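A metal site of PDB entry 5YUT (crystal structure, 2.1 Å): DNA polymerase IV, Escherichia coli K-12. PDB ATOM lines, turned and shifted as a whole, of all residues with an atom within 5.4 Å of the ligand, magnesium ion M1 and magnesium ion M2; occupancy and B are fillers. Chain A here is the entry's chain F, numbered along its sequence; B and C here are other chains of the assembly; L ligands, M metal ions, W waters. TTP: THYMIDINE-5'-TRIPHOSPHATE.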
ATOM      1  N   ASP A   9     -15.435  -6.386 -22.126  1.00  0.00           N
ATOM      2  CA  ASP A   9     -15.464  -6.628 -20.686  1.00  0.00           C
ATOM      3  C   ASP A   9     -14.461  -7.727 -20.368  1.00  0.00           C
ATOM      4  O   ASP A   9     -14.639  -8.860 -20.821  1.00  0.00           O
ATOM      5  CB  ASP A   9     -16.883  -7.036 -20.228  1.00  0.00           C
ATOM      6  CG  ASP A   9     -17.052  -7.013 -18.709  1.00  0.00           C
ATOM      7  OD1 ASP A   9     -16.104  -7.395 -18.013  1.00  0.00           O
ATOM      8  OD2 ASP A   9     -18.134  -6.614 -18.215  1.00  0.00           O
ATOM      9  N   MET A  10     -13.432  -7.408 -19.576  1.00  0.00           N
ATOM     10  CA  MET A  10     -12.426  -8.415 -19.205  1.00  0.00           C
ATOM     11  C   MET A  10     -13.038  -9.473 -18.295  1.00  0.00           C
ATOM     12  O   MET A  10     -13.909  -9.170 -17.457  1.00  0.00           O
ATOM     13  CB  MET A  10     -11.232  -7.759 -18.501  1.00  0.00           C
ATOM     14  CG  MET A  10     -10.555  -6.661 -19.298  1.00  0.00           C
ATOM     15  SD  MET A  10      -9.839  -7.224 -20.855  1.00  0.00           S
ATOM     16  CE  MET A  10      -8.540  -8.306 -20.240  1.00  0.00           C
ATOM     17  N   ASP A  11     -12.591 -10.721 -18.476  1.00  0.00           N
ATOM     18  CA  ASP A  11     -13.098 -11.859 -17.690  1.00  0.00           C
ATOM     19  C   ASP A  11     -12.395 -11.922 -16.340  1.00  0.00           C
ATOM     20  O   ASP A  11     -11.156 -11.965 -16.267  1.00  0.00           O
ATOM     21  CB  ASP A  11     -12.883 -13.174 -18.446  1.00  0.00           C
ATOM     22  CG  ASP A  11     -13.527 -13.198 -19.844  1.00  0.00           C
ATOM     23  OD1 ASP A  11     -14.701 -12.810 -19.997  1.00  0.00           O
ATOM     24  OD2 ASP A  11     -12.869 -13.635 -20.806  1.00  0.00           O
ATOM     25  N   CYS A  12     -13.186 -11.967 -15.257  1.00  0.00           N
ATOM     26  CA  CYS A  12     -12.674 -12.104 -13.883  1.00  0.00           C
ATOM     27  C   CYS A  12     -11.422 -11.257 -13.679  1.00  0.00           C
ATOM     28  O   CYS A  12     -10.363 -11.743 -13.274  1.00  0.00           O
ATOM     29  CB  CYS A  12     -12.392 -13.573 -13.541  1.00  0.00           C
ATOM     30  SG  CYS A  12     -13.812 -14.622 -13.789  1.00  0.00           S
ATOM     31  N   PHE A  13     -11.575  -9.956 -13.969  1.00  0.00           N
ATOM     32  CA  PHE A  13     -10.432  -9.111 -14.292  1.00  0.00           C
ATOM     33  C   PHE A  13      -9.312  -9.209 -13.246  1.00  0.00           C
ATOM     34  O   PHE A  13      -8.199  -9.648 -13.581  1.00  0.00           O
ATOM     35  CB  PHE A  13     -10.877  -7.662 -14.484  1.00  0.00           C
ATOM     36  CG  PHE A  13      -9.741  -6.739 -14.855  1.00  0.00           C
ATOM     37  CD1 PHE A  13      -8.813  -7.120 -15.808  1.00  0.00           C
ATOM     38  CD2 PHE A  13      -9.595  -5.514 -14.221  1.00  0.00           C
ATOM     39  CE1 PHE A  13      -7.756  -6.277 -16.155  1.00  0.00           C
ATOM     40  CE2 PHE A  13      -8.546  -4.658 -14.560  1.00  0.00           C
ATOM     41  CZ  PHE A  13      -7.619  -5.030 -15.516  1.00  0.00           C
ATOM     42  N   PHE A  14      -9.565  -8.795 -11.996  1.00  0.00           N
ATOM     43  CA  PHE A  14      -8.484  -8.797 -11.007  1.00  0.00           C
ATOM     44  C   PHE A  14      -7.896 -10.197 -10.873  1.00  0.00           C
ATOM     45  O   PHE A  14      -6.674 -10.383 -10.909  1.00  0.00           O
ATOM     46  CB  PHE A  14      -8.931  -8.322  -9.617  1.00  0.00           C
ATOM     47  CG  PHE A  14      -9.311  -6.884  -9.539  1.00  0.00           C
ATOM     48  CD1 PHE A  14      -9.279  -6.066 -10.651  1.00  0.00           C
ATOM     49  CD2 PHE A  14      -9.718  -6.346  -8.309  1.00  0.00           C
ATOM     50  CE1 PHE A  14      -9.660  -4.729 -10.559  1.00  0.00           C
ATOM     51  CE2 PHE A  14     -10.086  -5.006  -8.210  1.00  0.00           C
ATOM     52  CZ  PHE A  14     -10.068  -4.204  -9.336  1.00  0.00           C
ATOM     53  N   ALA A  15      -8.768 -11.203 -10.747  1.00  0.00           N
ATOM     54  CA  ALA A  15      -8.322 -12.587 -10.610  1.00  0.00           C
ATOM     55  C   ALA A  15      -7.570 -13.075 -11.855  1.00  0.00           C
ATOM     56  O   ALA A  15      -6.589 -13.812 -11.745  1.00  0.00           O
ATOM     57  CB  ALA A  15      -9.513 -13.503 -10.306  1.00  0.00           C
ATOM     58  N   ILE A  42     -15.611  -9.798  -1.069  1.00  0.00           N
ATOM     59  CA  ILE A  42     -14.922 -10.264  -2.275  1.00  0.00           C
ATOM     60  C   ILE A  42     -15.012  -9.176  -3.325  1.00  0.00           C
ATOM     61  O   ILE A  42     -16.107  -8.681  -3.608  1.00  0.00           O
ATOM     62  CB  ILE A  42     -15.565 -11.562  -2.787  1.00  0.00           C
ATOM     63  CG1 ILE A  42     -15.492 -12.656  -1.721  1.00  0.00           C
ATOM     64  CG2 ILE A  42     -14.905 -11.978  -4.092  1.00  0.00           C
ATOM     65  CD1 ILE A  42     -14.098 -12.964  -1.298  1.00  0.00           C
ATOM     66  N   SER A  43     -13.864  -8.800  -3.908  1.00  0.00           N
ATOM     67  CA  SER A  43     -13.910  -7.914  -5.060  1.00  0.00           C
ATOM     68  C   SER A  43     -14.262  -8.713  -6.316  1.00  0.00           C
ATOM     69  O   SER A  43     -15.135  -8.315  -7.098  1.00  0.00           O
ATOM     70  CB  SER A  43     -12.567  -7.194  -5.242  1.00  0.00           C
ATOM     71  OG  SER A  43     -12.560  -5.961  -4.538  1.00  0.00           O
ATOM     72  N   THR A  44     -13.561  -9.823  -6.523  1.00  0.00           N
ATOM     73  CA  THR A  44     -13.917 -10.765  -7.578  1.00  0.00           C
ATOM     74  C   THR A  44     -13.243 -12.096  -7.282  1.00  0.00           C
ATOM     75  O   THR A  44     -12.401 -12.185  -6.395  1.00  0.00           O
ATOM     76  CB  THR A  44     -13.532 -10.248  -8.964  1.00  0.00           C
ATOM     77  OG1 THR A  44     -14.166 -11.071  -9.946  1.00  0.00           O
ATOM     78  CG2 THR A  44     -12.047 -10.326  -9.180  1.00  0.00           C
ATOM     79  N   ALA A  45     -13.641 -13.116  -8.030  1.00  0.00           N
ATOM     80  CA  ALA A  45     -13.164 -14.472  -7.845  1.00  0.00           C
ATOM     81  C   ALA A  45     -12.931 -15.105  -9.209  1.00  0.00           C
ATOM     82  O   ALA A  45     -13.482 -14.677 -10.222  1.00  0.00           O
ATOM     83  CB  ALA A  45     -14.167 -15.305  -7.037  1.00  0.00           C
ATOM     84  N   TYR A  47     -12.961 -18.667 -11.734  1.00  0.00           N
ATOM     85  CA  TYR A  47     -14.046 -19.630 -11.955  1.00  0.00           C
ATOM     86  C   TYR A  47     -14.008 -20.825 -10.997  1.00  0.00           C
ATOM     87  O   TYR A  47     -15.075 -21.288 -10.553  1.00  0.00           O
ATOM     88  CB  TYR A  47     -14.062 -20.084 -13.414  1.00  0.00           C
ATOM     89  CG  TYR A  47     -14.853 -19.098 -14.279  1.00  0.00           C
ATOM     90  CD1 TYR A  47     -16.236 -19.126 -14.296  1.00  0.00           C
ATOM     91  CD2 TYR A  47     -14.219 -18.099 -15.021  1.00  0.00           C
ATOM     92  CE1 TYR A  47     -16.975 -18.207 -15.050  1.00  0.00           C
ATOM     93  CE2 TYR A  47     -14.951 -17.183 -15.787  1.00  0.00           C
ATOM     94  CZ  TYR A  47     -16.322 -17.250 -15.793  1.00  0.00           C
ATOM     95  OH  TYR A  47     -17.091 -16.380 -16.535  1.00  0.00           O
ATOM     96  N   ARG A  50     -15.892 -19.354  -8.089  1.00  0.00           N
ATOM     97  CA  ARG A  50     -17.276 -19.124  -8.498  1.00  0.00           C
ATOM     98  C   ARG A  50     -18.093 -20.409  -8.514  1.00  0.00           C
ATOM     99  O   ARG A  50     -19.297 -20.375  -8.213  1.00  0.00           O
ATOM    100  CB  ARG A  50     -17.325 -18.466  -9.884  1.00  0.00           C
ATOM    101  CG  ARG A  50     -16.869 -17.045  -9.860  1.00  0.00           C
ATOM    102  CD  ARG A  50     -16.831 -16.353 -11.221  1.00  0.00           C
ATOM    103  NE  ARG A  50     -16.374 -14.987 -10.984  1.00  0.00           N
ATOM    104  CZ  ARG A  50     -16.382 -13.997 -11.866  1.00  0.00           C
ATOM    105  NH1 ARG A  50     -16.825 -14.202 -13.104  1.00  0.00           N
ATOM    106  NH2 ARG A  50     -15.933 -12.806 -11.491  1.00  0.00           N
ATOM    107  N   SER A  56     -18.648 -11.514  -6.431  1.00  0.00           N
ATOM    108  CA  SER A  56     -18.336 -10.129  -6.061  1.00  0.00           C
ATOM    109  C   SER A  56     -19.365  -9.593  -5.075  1.00  0.00           C
ATOM    110  O   SER A  56     -20.554  -9.919  -5.150  1.00  0.00           O
ATOM    111  CB  SER A  56     -18.327  -9.217  -7.298  1.00  0.00           C
ATOM    112  OG  SER A  56     -17.322  -9.585  -8.218  1.00  0.00           O
ATOM    113  N   ALA A  57     -18.895  -8.753  -4.150  1.00  0.00           N
ATOM    114  CA  ALA A  57     -19.707  -8.089  -3.126  1.00  0.00           C
ATOM    115  C   ALA A  57     -20.143  -9.033  -2.024  1.00  0.00           C
ATOM    116  O   ALA A  57     -20.827  -8.604  -1.086  1.00  0.00           O
ATOM    117  CB  ALA A  57     -20.939  -7.385  -3.711  1.00  0.00           C
ATOM    118  N   SER A 102     -14.873   1.610 -16.406  1.00  0.00           N
ATOM    119  CA  SER A 102     -14.126   1.169 -15.235  1.00  0.00           C
ATOM    120  C   SER A 102     -12.774   0.712 -15.745  1.00  0.00           C
ATOM    121  O   SER A 102     -12.505   0.833 -16.947  1.00  0.00           O
ATOM    122  CB  SER A 102     -14.850   0.034 -14.512  1.00  0.00           C
ATOM    123  OG  SER A 102     -15.060  -1.081 -15.376  1.00  0.00           O
ATOM    124  N   ASP A 104     -11.801  -2.239 -16.398  1.00  0.00           N
ATOM    125  CA  ASP A 104     -11.781  -3.439 -17.227  1.00  0.00           C
ATOM    126  C   ASP A 104     -12.794  -3.438 -18.382  1.00  0.00           C
ATOM    127  O   ASP A 104     -12.956  -4.485 -19.020  1.00  0.00           O
ATOM    128  CB  ASP A 104     -11.983  -4.676 -16.333  1.00  0.00           C
ATOM    129  CG  ASP A 104     -13.445  -5.064 -16.186  1.00  0.00           C
ATOM    130  OD1 ASP A 104     -14.340  -4.198 -16.144  1.00  0.00           O
ATOM    131  OD2 ASP A 104     -13.682  -6.297 -16.117  1.00  0.00           O
ATOM    132  N   GLU A 105     -13.453  -2.316 -18.674  1.00  0.00           N
ATOM    133  CA  GLU A 105     -14.489  -2.353 -19.691  1.00  0.00           C
ATOM    134  C   GLU A 105     -14.677  -1.002 -20.358  1.00  0.00           C
ATOM    135  O   GLU A 105     -14.348   0.046 -19.799  1.00  0.00           O
ATOM    136  CB  GLU A 105     -15.820  -2.901 -19.128  1.00  0.00           C
ATOM    137  CG  GLU A 105     -16.625  -1.986 -18.204  1.00  0.00           C
ATOM    138  CD  GLU A 105     -17.923  -2.637 -17.666  1.00  0.00           C
ATOM    139  OE1 GLU A 105     -17.848  -3.658 -16.949  1.00  0.00           O
ATOM    140  OE2 GLU A 105     -19.016  -2.129 -17.943  1.00  0.00           O
ATOM    141  N   ASP A 155     -22.225 -10.244 -21.465  1.00  0.00           N
ATOM    142  CA  ASP A 155     -22.316 -11.197 -20.369  1.00  0.00           C
ATOM    143  C   ASP A 155     -22.734 -12.580 -20.814  1.00  0.00           C
ATOM    144  O   ASP A 155     -22.591 -13.533 -20.027  1.00  0.00           O
ATOM    145  CB  ASP A 155     -23.323 -10.724 -19.323  1.00  0.00           C
ATOM    146  CG  ASP A 155     -22.715  -9.868 -18.271  1.00  0.00           C
ATOM    147  OD1 ASP A 155     -21.463  -9.741 -18.260  1.00  0.00           O
ATOM    148  OD2 ASP A 155     -23.483  -9.318 -17.465  1.00  0.00           O
ATOM    149  N   LYS A 158     -19.706 -15.140 -21.860  1.00  0.00           N
ATOM    150  CA  LYS A 158     -18.567 -15.110 -20.938  1.00  0.00           C
ATOM    151  C   LYS A 158     -18.275 -16.513 -20.405  1.00  0.00           C
ATOM    152  O   LYS A 158     -19.199 -17.247 -20.124  1.00  0.00           O
ATOM    153  CB  LYS A 158     -18.848 -14.189 -19.750  1.00  0.00           C
ATOM    154  CG  LYS A 158     -18.404 -12.786 -19.933  1.00  0.00           C
ATOM    155  CD  LYS A 158     -18.656 -11.933 -18.696  1.00  0.00           C
ATOM    156  CE  LYS A 158     -17.994 -10.555 -18.852  1.00  0.00           C
ATOM    157  NZ  LYS A 158     -16.474 -10.648 -18.898  1.00  0.00           N
ATOM    158  P    DC B  18     -21.807  -3.245 -13.649  1.00  0.00           P
ATOM    159  OP1  DC B  18     -21.843  -3.798 -14.994  1.00  0.00           O
ATOM    160  OP2  DC B  18     -22.369  -4.052 -12.535  1.00  0.00           O
ATOM    161  O5'  DC B  18     -20.262  -2.957 -13.228  1.00  0.00           O
ATOM    162  C5'  DC B  18     -19.488  -1.961 -13.935  1.00  0.00           C
ATOM    163  C4'  DC B  18     -18.103  -1.856 -13.318  1.00  0.00           C
ATOM    164  O4'  DC B  18     -18.181  -1.165 -12.051  1.00  0.00           O
ATOM    165  C3'  DC B  18     -17.442  -3.203 -13.035  1.00  0.00           C
ATOM    166  O3'  DC B  18     -16.579  -3.517 -14.062  1.00  0.00           O
ATOM    167  C2'  DC B  18     -16.681  -2.987 -11.740  1.00  0.00           C
ATOM    168  C1'  DC B  18     -17.302  -1.764 -11.114  1.00  0.00           C
ATOM    169  N1   DC B  18     -18.040  -2.007  -9.844  1.00  0.00           N
ATOM    170  C2   DC B  18     -17.363  -1.850  -8.651  1.00  0.00           C
ATOM    171  O2   DC B  18     -16.144  -1.568  -8.676  1.00  0.00           O
ATOM    172  N3   DC B  18     -18.037  -1.998  -7.482  1.00  0.00           N
ATOM    173  C4   DC B  18     -19.333  -2.314  -7.483  1.00  0.00           C
ATOM    174  N4   DC B  18     -19.931  -2.451  -6.291  1.00  0.00           N
ATOM    175  C5   DC B  18     -20.057  -2.501  -8.699  1.00  0.00           C
ATOM    176  C6   DC B  18     -19.370  -2.328  -9.857  1.00  0.00           C
ATOM    177  P    DA C   4     -18.656  -3.775   4.082  1.00  0.00           P
ATOM    178  OP1  DA C   4     -18.478  -3.315   5.483  1.00  0.00           O
ATOM    179  OP2  DA C   4     -19.660  -3.068   3.263  1.00  0.00           O
ATOM    180  O5'  DA C   4     -17.305  -3.743   3.241  1.00  0.00           O
ATOM    181  C5'  DA C   4     -16.143  -4.339   3.717  1.00  0.00           C
ATOM    182  C4'  DA C   4     -14.932  -3.738   3.010  1.00  0.00           C
ATOM    183  O4'  DA C   4     -14.946  -4.071   1.594  1.00  0.00           O
ATOM    184  C3'  DA C   4     -14.832  -2.222   3.077  1.00  0.00           C
ATOM    185  O3'  DA C   4     -13.464  -1.825   3.121  1.00  0.00           O
ATOM    186  C2'  DA C   4     -15.506  -1.763   1.766  1.00  0.00           C
ATOM    187  C1'  DA C   4     -15.174  -2.910   0.808  1.00  0.00           C
ATOM    188  N9   DA C   4     -16.258  -3.220  -0.105  1.00  0.00           N
ATOM    189  C8   DA C   4     -17.593  -3.224   0.162  1.00  0.00           C
ATOM    190  N7   DA C   4     -18.334  -3.570  -0.865  1.00  0.00           N
ATOM    191  C5   DA C   4     -17.422  -3.809  -1.864  1.00  0.00           C
ATOM    192  C6   DA C   4     -17.578  -4.210  -3.215  1.00  0.00           C
ATOM    193  N6   DA C   4     -18.763  -4.450  -3.784  1.00  0.00           N
ATOM    194  N1   DA C   4     -16.454  -4.370  -3.941  1.00  0.00           N
ATOM    195  C2   DA C   4     -15.265  -4.123  -3.353  1.00  0.00           C
ATOM    196  N3   DA C   4     -15.008  -3.743  -2.104  1.00  0.00           N
ATOM    197  C4   DA C   4     -16.139  -3.605  -1.411  1.00  0.00           C
ATOM    198  P    DG C   5     -13.077  -0.284   3.290  1.00  0.00           P
ATOM    199  OP1  DG C   5     -11.776  -0.305   4.012  1.00  0.00           O
ATOM    200  OP2  DG C   5     -14.260   0.467   3.834  1.00  0.00           O
ATOM    201  O5'  DG C   5     -12.853   0.218   1.814  1.00  0.00           O
ATOM    202  C5'  DG C   5     -11.773  -0.276   1.074  1.00  0.00           C
ATOM    203  C4'  DG C   5     -11.750   0.404  -0.259  1.00  0.00           C
ATOM    204  O4'  DG C   5     -12.800  -0.131  -1.122  1.00  0.00           O
ATOM    205  C3'  DG C   5     -11.995   1.911  -0.179  1.00  0.00           C
ATOM    206  O3'  DG C   5     -11.156   2.516  -1.110  1.00  0.00           O
ATOM    207  C2'  DG C   5     -13.465   2.060  -0.596  1.00  0.00           C
ATOM    208  C1'  DG C   5     -13.584   0.938  -1.617  1.00  0.00           C
ATOM    209  N9   DG C   5     -14.956   0.492  -1.869  1.00  0.00           N
ATOM    210  C8   DG C   5     -16.035   0.560  -1.013  1.00  0.00           C
ATOM    211  N7   DG C   5     -17.136   0.097  -1.533  1.00  0.00           N
ATOM    212  C5   DG C   5     -16.768  -0.314  -2.820  1.00  0.00           C
ATOM    213  C6   DG C   5     -17.540  -0.900  -3.865  1.00  0.00           C
ATOM    214  O6   DG C   5     -18.744  -1.212  -3.866  1.00  0.00           O
ATOM    215  N1   DG C   5     -16.767  -1.156  -4.991  1.00  0.00           N
ATOM    216  C2   DG C   5     -15.444  -0.877  -5.102  1.00  0.00           C
ATOM    217  N2   DG C   5     -14.877  -1.201  -6.278  1.00  0.00           N
ATOM    218  N3   DG C   5     -14.713  -0.326  -4.154  1.00  0.00           N
ATOM    219  C4   DG C   5     -15.437  -0.081  -3.036  1.00  0.00           C
HETATM  220  PA  TTP L   1     -16.652  -6.861 -13.381  1.00  0.00           P
HETATM  221  O1A TTP L   1     -16.408  -6.904 -14.877  1.00  0.00           O
HETATM  222  O2A TTP L   1     -18.072  -6.548 -12.980  1.00  0.00           O
HETATM  223  O3A TTP L   1     -16.394  -8.345 -12.802  1.00  0.00           O
HETATM  224  PB  TTP L   1     -15.251  -9.347 -13.305  1.00  0.00           P
HETATM  225  O1B TTP L   1     -14.360  -9.750 -12.135  1.00  0.00           O
HETATM  226  O2B TTP L   1     -14.368  -8.840 -14.405  1.00  0.00           O
HETATM  227  O3B TTP L   1     -16.147 -10.608 -13.710  1.00  0.00           O
HETATM  228  PG  TTP L   1     -16.687 -10.905 -15.209  1.00  0.00           P
HETATM  229  O1G TTP L   1     -16.783  -9.635 -16.062  1.00  0.00           O
HETATM  230  O2G TTP L   1     -18.067 -11.468 -14.933  1.00  0.00           O
HETATM  231  O3G TTP L   1     -15.786 -11.940 -15.842  1.00  0.00           O
HETATM  232  O5' TTP L   1     -15.630  -5.939 -12.560  1.00  0.00           O
HETATM  233  C5' TTP L   1     -14.264  -5.754 -12.951  1.00  0.00           C
HETATM  234  C4' TTP L   1     -13.418  -5.718 -11.665  1.00  0.00           C
HETATM  235  O4' TTP L   1     -13.962  -4.740 -10.775  1.00  0.00           O
HETATM  236  C3' TTP L   1     -13.483  -7.032 -10.892  1.00  0.00           C
HETATM  237  O3' TTP L   1     -12.568  -8.034 -11.366  1.00  0.00           O
HETATM  238  C2' TTP L   1     -13.216  -6.577  -9.454  1.00  0.00           C
HETATM  239  C1' TTP L   1     -13.817  -5.177  -9.401  1.00  0.00           C
HETATM  240  N1  TTP L   1     -15.134  -5.228  -8.744  1.00  0.00           N
HETATM  241  C2  TTP L   1     -15.202  -4.944  -7.370  1.00  0.00           C
HETATM  242  O2  TTP L   1     -14.150  -4.624  -6.767  1.00  0.00           O
HETATM  243  N3  TTP L   1     -16.375  -4.977  -6.707  1.00  0.00           N
HETATM  244  C4  TTP L   1     -17.504  -5.330  -7.335  1.00  0.00           C
HETATM  245  O4  TTP L   1     -18.598  -5.381  -6.736  1.00  0.00           O
HETATM  246  C5  TTP L   1     -17.471  -5.667  -8.770  1.00  0.00           C
HETATM  247  C5M TTP L   1     -18.757  -6.058  -9.460  1.00  0.00           C
HETATM  248  C6  TTP L   1     -16.234  -5.608  -9.424  1.00  0.00           C
HETATM  249 MG    MG M   1     -15.304  -7.909 -16.224  1.00  0.00          MG
HETATM  250 MG    MG M   2     -16.605  -4.774 -16.051  1.00  0.00          MG
HETATM  251  O   HOH W   1     -21.320  -5.570  -7.037  1.00  0.00           O
HETATM  252  O   HOH W   2     -15.739 -14.142 -17.291  1.00  0.00           O
HETATM  253  O   HOH W   3     -19.099  -5.866 -16.053  1.00  0.00           O
HETATM  254  O   HOH W   4     -19.584 -11.390 -12.625  1.00  0.00           O
HETATM  255  O   HOH W   5     -18.040 -10.400 -10.664  1.00  0.00           O
HETATM  256  O   HOH W   6     -19.220  -8.345 -16.181  1.00  0.00           O
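N3 of DC 18 of chain B lies close to N3 of the ligand (3.5 Å). OG1 of Thr 44 is in hydrogen-bond range of O1B of the ligand (2.6 Å). O3G of the ligand lies within hydrogen-bond range of N of Cys 12, 2.7 Å away. N1 of DA 4 of chain C is in hydrogen-bond range of N3 of the ligand (2.8 Å). O3G of the ligand is in salt-bridge range of NZ of Lys 158, at 3.4 Å. N of Phe 13 lies within hydrogen-bond range of O1B of the ligand (3.3 Å). An oxygen (O2) of the ligand is in hydrogen-bond range of the side-chain hydroxyl (OG) of Ser 43 (3.0 Å). The guanidinium group (NH2) of Arg 50 is in salt-bridge range of an oxygen (O1B) of the ligand, 3.5 Å away. The backbone NH of Phe 14 is in hydrogen-bond range of an oxygen (O3') of the ligand, 3.2 Å away.
The backbone carbonyl oxygen of Asp 9 sits at hydrogen-bond distance from the side-chain amino group of Lys 158 (3.2 Å). NZ of Lys 158 lies close to O of Met 10, 3.3 Å away. OD1 of Asp 104 sits close to OG of Ser 102. N2 of DG 5 of chain C lies close to O2 of DC 18 of chain B, 2.7 Å away. The guanidinium group of Arg 50 lies within hydrogen-bond range of the side-chain hydroxyl of Thr 44 (2.9 Å). The guanidinium group (NH1) of Arg 50 sits at hydrogen-bond distance from the side-chain sulfur (SG) of Cys 12 (3.1 Å). O of Ser 43 sits at hydrogen-bond distance from OG of Ser 56, 2.8 Å away. O of Ala 45 lies within hydrogen-bond range of NE of Arg 50 (3.0 Å).
Asp 11 touches the ligand. CB of Ser 56 touches C5M of the ligand, at 3.9 Å. DG 5 of chain C touches the ligand (N2 to O2, 3.5 Å). Hydrophobic or aromatic side chains that line the ligand: Phe 13 and Phe 14. Within 4 Å of the ligand: Asp 9, Met 10, Asp 11, Cys 12, Phe 13, Phe 14, Ser 43, Thr 44, Arg 50, Ser 56, Asp 104, Lys 158, DC 18 of chain B, DA 4 of chain C and DG 5 of chain C. Along chain A the residues within 4 Å of the ligand span positions 9 to 158.
Three residues have an atom within 4 Å of magnesium ion M1: Asp 9, Met 10 and Asp 104. The nearest printed residue that does not touch magnesium ion M1 is Lys 158 (4.003 Å).
Magnesium ion M1 is bound by an oxygen (O1A) of the ligand, the side-chain carboxylate (OD1) of Asp 9, an oxygen (O2B) of the ligand, the backbone carbonyl oxygen (O) of Met 10, an oxygen (O1G) of the ligand and the side-chain carboxylate (OD2) of Asp 104.
Magnesium ion M2 is bound by OE1 of Glu 105 (1.9 Å), OD1 of Asp 104 (2.3 Å), O3' of DC 18 of chain B (2.4 Å) and O1A of the ligand (2.4 Å). Slightly farther from magnesium ion M2 lies water W3 (2.7 Å).
Water W3 lies within hydrogen-bond range of OD2 of Asp 9 (2.5 Å) and O2A of the ligand (3.3 Å). Water W2 lies within hydrogen-bond range of O3G of the ligand (2.6 Å), OH of Tyr 47 (2.7 Å) and OD1 of Asp 11 (3.2 Å). Water W1 lies within hydrogen-bond range of O4 of the ligand and N4 of DC 18 of chain B. Water W6 bridges the side-chain carboxylate (OD2) of Asp 9 (2.9 Å) and the side-chain carboxylate (OD1) of Asp 155 (3.4 Å). Water W5 lies within hydrogen-bond range of OG of Ser 56, NH2 of Arg 50 and O3A of the ligand.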
